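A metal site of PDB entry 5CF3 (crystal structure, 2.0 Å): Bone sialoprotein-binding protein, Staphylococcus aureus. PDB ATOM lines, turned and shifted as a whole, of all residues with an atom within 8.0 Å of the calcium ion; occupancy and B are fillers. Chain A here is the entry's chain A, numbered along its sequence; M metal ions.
The side-chain carboxylate (OE2) of Glu 21 sits at hydrogen-bond distance from the backbone NH (N) of Gly 27 (2.9 Å). OD2 of Asp 25 is in hydrogen-bond range of N of Glu 21, at 3.2 Å. The side-chain carboxylate of Asp 26 sits close to the side-chain amide nitrogen of Gln 30 (3.2 Å). The backbone NH (N) of Ile 23 lies close to the side-chain carboxylate (OE1) of Glu 35. The backbone NH (N) of Glu 35 lies within hydrogen-bond range of the backbone carbonyl oxygen (O) of Gln 30 (3.2 Å).
The nearest printed residue that does not touch the calcium ion is Gln 30 (4.1 Å).
O of Val 28 binds the calcium ion (2.3 Å). The calcium ion is bound by the side-chain carboxylate (OE1) of Glu 35. The side-chain carboxylate (OE1) of Glu 21 binds the calcium ion, 2.4 Å away. The calcium ion is bound by O of Lys 24. The calcium ion is bound by the side-chain carboxylate (OE2) of Glu 35, at 2.6 Å. The calcium ion is bound by OD2 of Asp 26.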
ATOM      1  N   THR A  20     -11.346  22.303  -9.408  1.00  0.00           N
ATOM      2  CA  THR A  20     -11.990  22.334  -8.095  1.00  0.00           C
ATOM      3  C   THR A  20     -12.080  20.921  -7.485  1.00  0.00           C
ATOM      4  O   THR A  20     -11.690  19.940  -8.128  1.00  0.00           O
ATOM      5  CB  THR A  20     -13.379  22.992  -8.175  1.00  0.00           C
ATOM      6  OG1 THR A  20     -14.235  22.220  -9.025  1.00  0.00           O
ATOM      7  CG2 THR A  20     -13.262  24.392  -8.750  1.00  0.00           C
ATOM      8  N   GLU A  21     -12.584  20.827  -6.254  1.00  0.00           N
ATOM      9  CA  GLU A  21     -12.619  19.556  -5.546  1.00  0.00           C
ATOM     10  C   GLU A  21     -14.043  19.108  -5.263  1.00  0.00           C
ATOM     11  O   GLU A  21     -14.960  19.918  -5.188  1.00  0.00           O
ATOM     12  CB  GLU A  21     -11.840  19.644  -4.240  1.00  0.00           C
ATOM     13  CG  GLU A  21     -10.432  20.150  -4.433  1.00  0.00           C
ATOM     14  CD  GLU A  21      -9.784  20.586  -3.147  1.00  0.00           C
ATOM     15  OE1 GLU A  21      -9.602  19.745  -2.248  1.00  0.00           O
ATOM     16  OE2 GLU A  21      -9.418  21.777  -3.042  1.00  0.00           O
ATOM     17  N   GLY A  22     -14.221  17.800  -5.116  1.00  0.00           N
ATOM     18  CA  GLY A  22     -15.543  17.214  -4.993  1.00  0.00           C
ATOM     19  C   GLY A  22     -16.193  17.282  -3.614  1.00  0.00           C
ATOM     20  O   GLY A  22     -17.412  17.189  -3.510  1.00  0.00           O
ATOM     21  N   ILE A  23     -15.400  17.420  -2.555  1.00  0.00           N
ATOM     22  CA  ILE A  23     -15.942  17.333  -1.197  1.00  0.00           C
ATOM     23  C   ILE A  23     -15.809  18.666  -0.481  1.00  0.00           C
ATOM     24  O   ILE A  23     -16.797  19.209   0.003  1.00  0.00           O
ATOM     25  CB  ILE A  23     -15.243  16.255  -0.342  1.00  0.00           C
ATOM     26  CG1 ILE A  23     -15.542  14.864  -0.890  1.00  0.00           C
ATOM     27  CG2 ILE A  23     -15.684  16.363   1.119  1.00  0.00           C
ATOM     28  CD1 ILE A  23     -14.801  13.746  -0.140  1.00  0.00           C
ATOM     29  N   LYS A  24     -14.594  19.166  -0.406  1.00  0.00           N
ATOM     30  CA  LYS A  24     -14.339  20.426   0.265  1.00  0.00           C
ATOM     31  C   LYS A  24     -13.153  21.087  -0.410  1.00  0.00           C
ATOM     32  O   LYS A  24     -12.110  20.455  -0.577  1.00  0.00           O
ATOM     33  CB  LYS A  24     -14.097  20.189   1.759  1.00  0.00           C
ATOM     34  CG  LYS A  24     -13.797  21.419   2.608  1.00  0.00           C
ATOM     35  CD  LYS A  24     -13.623  21.006   4.073  1.00  0.00           C
ATOM     36  CE  LYS A  24     -13.087  22.140   4.946  1.00  0.00           C
ATOM     37  NZ  LYS A  24     -14.110  23.154   5.339  1.00  0.00           N
ATOM     38  N   ASP A  25     -13.295  22.347  -0.810  1.00  0.00           N
ATOM     39  CA  ASP A  25     -12.205  22.988  -1.528  1.00  0.00           C
ATOM     40  C   ASP A  25     -11.052  23.261  -0.549  1.00  0.00           C
ATOM     41  O   ASP A  25     -10.828  24.384  -0.110  1.00  0.00           O
ATOM     42  CB  ASP A  25     -12.690  24.241  -2.255  1.00  0.00           C
ATOM     43  CG  ASP A  25     -13.407  23.906  -3.568  1.00  0.00           C
ATOM     44  OD1 ASP A  25     -14.645  24.054  -3.637  1.00  0.00           O
ATOM     45  OD2 ASP A  25     -12.738  23.466  -4.525  1.00  0.00           O
ATOM     46  N   ASP A  26     -10.334  22.179  -0.254  1.00  0.00           N
ATOM     47  CA  ASP A  26      -9.318  22.076   0.782  1.00  0.00           C
ATOM     48  C   ASP A  26      -7.918  22.492   0.366  1.00  0.00           C
ATOM     49  O   ASP A  26      -7.137  22.990   1.173  1.00  0.00           O
ATOM     50  CB  ASP A  26      -9.232  20.619   1.250  1.00  0.00           C
ATOM     51  CG  ASP A  26     -10.318  20.242   2.215  1.00  0.00           C
ATOM     52  OD1 ASP A  26     -10.607  21.062   3.109  1.00  0.00           O
ATOM     53  OD2 ASP A  26     -10.886  19.133   2.080  1.00  0.00           O
ATOM     54  N   GLY A  27      -7.581  22.217  -0.899  1.00  0.00           N
ATOM     55  CA  GLY A  27      -6.184  22.148  -1.302  1.00  0.00           C
ATOM     56  C   GLY A  27      -5.657  20.795  -0.875  1.00  0.00           C
ATOM     57  O   GLY A  27      -4.477  20.491  -1.023  1.00  0.00           O
ATOM     58  N   VAL A  28      -6.547  19.974  -0.324  1.00  0.00           N
ATOM     59  CA  VAL A  28      -6.221  18.642   0.152  1.00  0.00           C
ATOM     60  C   VAL A  28      -7.200  17.635  -0.449  1.00  0.00           C
ATOM     61  O   VAL A  28      -8.413  17.736  -0.234  1.00  0.00           O
ATOM     62  CB  VAL A  28      -6.277  18.561   1.693  1.00  0.00           C
ATOM     63  CG1 VAL A  28      -5.923  17.165   2.173  1.00  0.00           C
ATOM     64  CG2 VAL A  28      -5.376  19.606   2.310  1.00  0.00           C
ATOM     65  N   ILE A  29      -6.686  16.662  -1.188  1.00  0.00           N
ATOM     66  CA  ILE A  29      -7.555  15.669  -1.805  1.00  0.00           C
ATOM     67  C   ILE A  29      -7.717  14.451  -0.928  1.00  0.00           C
ATOM     68  O   ILE A  29      -6.742  13.730  -0.641  1.00  0.00           O
ATOM     69  CB  ILE A  29      -7.035  15.211  -3.187  1.00  0.00           C
ATOM     70  CG1 ILE A  29      -6.669  16.402  -4.078  1.00  0.00           C
ATOM     71  CG2 ILE A  29      -8.084  14.321  -3.841  1.00  0.00           C
ATOM     72  CD1 ILE A  29      -7.834  17.289  -4.411  1.00  0.00           C
ATOM     73  N   GLN A  30      -8.947  14.180  -0.502  1.00  0.00           N
ATOM     74  CA  GLN A  30      -9.206  13.008   0.338  1.00  0.00           C
ATOM     75  C   GLN A  30      -9.406  11.773  -0.537  1.00  0.00           C
ATOM     76  O   GLN A  30     -10.526  11.336  -0.754  1.00  0.00           O
ATOM     77  CB  GLN A  30     -10.416  13.226   1.249  1.00  0.00           C
ATOM     78  CG  GLN A  30     -10.394  14.540   2.049  1.00  0.00           C
ATOM     79  CD  GLN A  30     -11.774  14.934   2.624  1.00  0.00           C
ATOM     80  OE1 GLN A  30     -12.568  14.072   3.024  1.00  0.00           O
ATOM     81  NE2 GLN A  30     -12.058  16.236   2.653  1.00  0.00           N
ATOM     82  N   ALA A  31      -8.298  11.208  -1.035  1.00  0.00           N
ATOM     83  CA  ALA A  31      -8.376  10.173  -2.062  1.00  0.00           C
ATOM     84  C   ALA A  31      -9.103   8.918  -1.578  1.00  0.00           C
ATOM     85  O   ALA A  31      -9.786   8.241  -2.351  1.00  0.00           O
ATOM     86  CB  ALA A  31      -6.987   9.804  -2.564  1.00  0.00           C
ATOM     87  N   GLU A  35     -12.640  11.602  -3.167  1.00  0.00           N
ATOM     88  CA  GLU A  35     -12.833  13.006  -3.510  1.00  0.00           C
ATOM     89  C   GLU A  35     -12.432  13.286  -4.955  1.00  0.00           C
ATOM     90  O   GLU A  35     -11.273  13.101  -5.335  1.00  0.00           O
ATOM     91  CB  GLU A  35     -12.041  13.932  -2.590  1.00  0.00           C
ATOM     92  CG  GLU A  35     -12.386  15.391  -2.840  1.00  0.00           C
ATOM     93  CD  GLU A  35     -11.779  16.348  -1.833  1.00  0.00           C
ATOM     94  OE1 GLU A  35     -12.292  17.482  -1.722  1.00  0.00           O
ATOM     95  OE2 GLU A  35     -10.795  15.978  -1.175  1.00  0.00           O
ATOM     96  N   HIS A  36     -13.392  13.764  -5.739  1.00  0.00           N
ATOM     97  CA  HIS A  36     -13.139  14.164  -7.125  1.00  0.00           C
ATOM     98  C   HIS A  36     -12.186  15.341  -7.264  1.00  0.00           C
ATOM     99  O   HIS A  36     -12.207  16.271  -6.480  1.00  0.00           O
ATOM    100  CB  HIS A  36     -14.452  14.525  -7.809  1.00  0.00           C
ATOM    101  CG  HIS A  36     -15.337  13.355  -8.073  1.00  0.00           C
ATOM    102  ND1 HIS A  36     -16.704  13.426  -7.966  1.00  0.00           N
ATOM    103  CD2 HIS A  36     -15.051  12.084  -8.458  1.00  0.00           C
ATOM    104  CE1 HIS A  36     -17.232  12.244  -8.255  1.00  0.00           C
ATOM    105  NE2 HIS A  36     -16.242  11.419  -8.551  1.00  0.00           N
ATOM    106  N   VAL A 147      -2.057  20.913  -4.752  1.00  0.00           N
ATOM    107  CA  VAL A 147      -2.847  20.216  -3.754  1.00  0.00           C
ATOM    108  C   VAL A 147      -1.986  19.291  -2.915  1.00  0.00           C
ATOM    109  O   VAL A 147      -0.825  19.021  -3.253  1.00  0.00           O
ATOM    110  CB  VAL A 147      -3.985  19.386  -4.390  1.00  0.00           C
ATOM    111  CG1 VAL A 147      -4.997  20.280  -5.071  1.00  0.00           C
ATOM    112  CG2 VAL A 147      -3.420  18.366  -5.362  1.00  0.00           C
ATOM    113  N   LYS A 148      -2.551  18.814  -1.816  1.00  0.00           N
ATOM    114  CA  LYS A 148      -1.955  17.751  -1.036  1.00  0.00           C
ATOM    115  C   LYS A 148      -2.860  16.533  -1.165  1.00  0.00           C
ATOM    116  O   LYS A 148      -4.079  16.649  -1.066  1.00  0.00           O
ATOM    117  CB  LYS A 148      -1.784  18.141   0.440  1.00  0.00           C
ATOM    118  CG  LYS A 148      -0.897  19.366   0.659  1.00  0.00           C
ATOM    119  CD  LYS A 148      -0.132  19.305   1.984  1.00  0.00           C
ATOM    120  CE  LYS A 148      -0.899  19.954   3.129  1.00  0.00           C
ATOM    121  NZ  LYS A 148      -1.699  18.969   3.927  1.00  0.00           N
HETATM  122 CA    CA M   1     -10.589  18.514  -0.489  1.00  0.00          CA
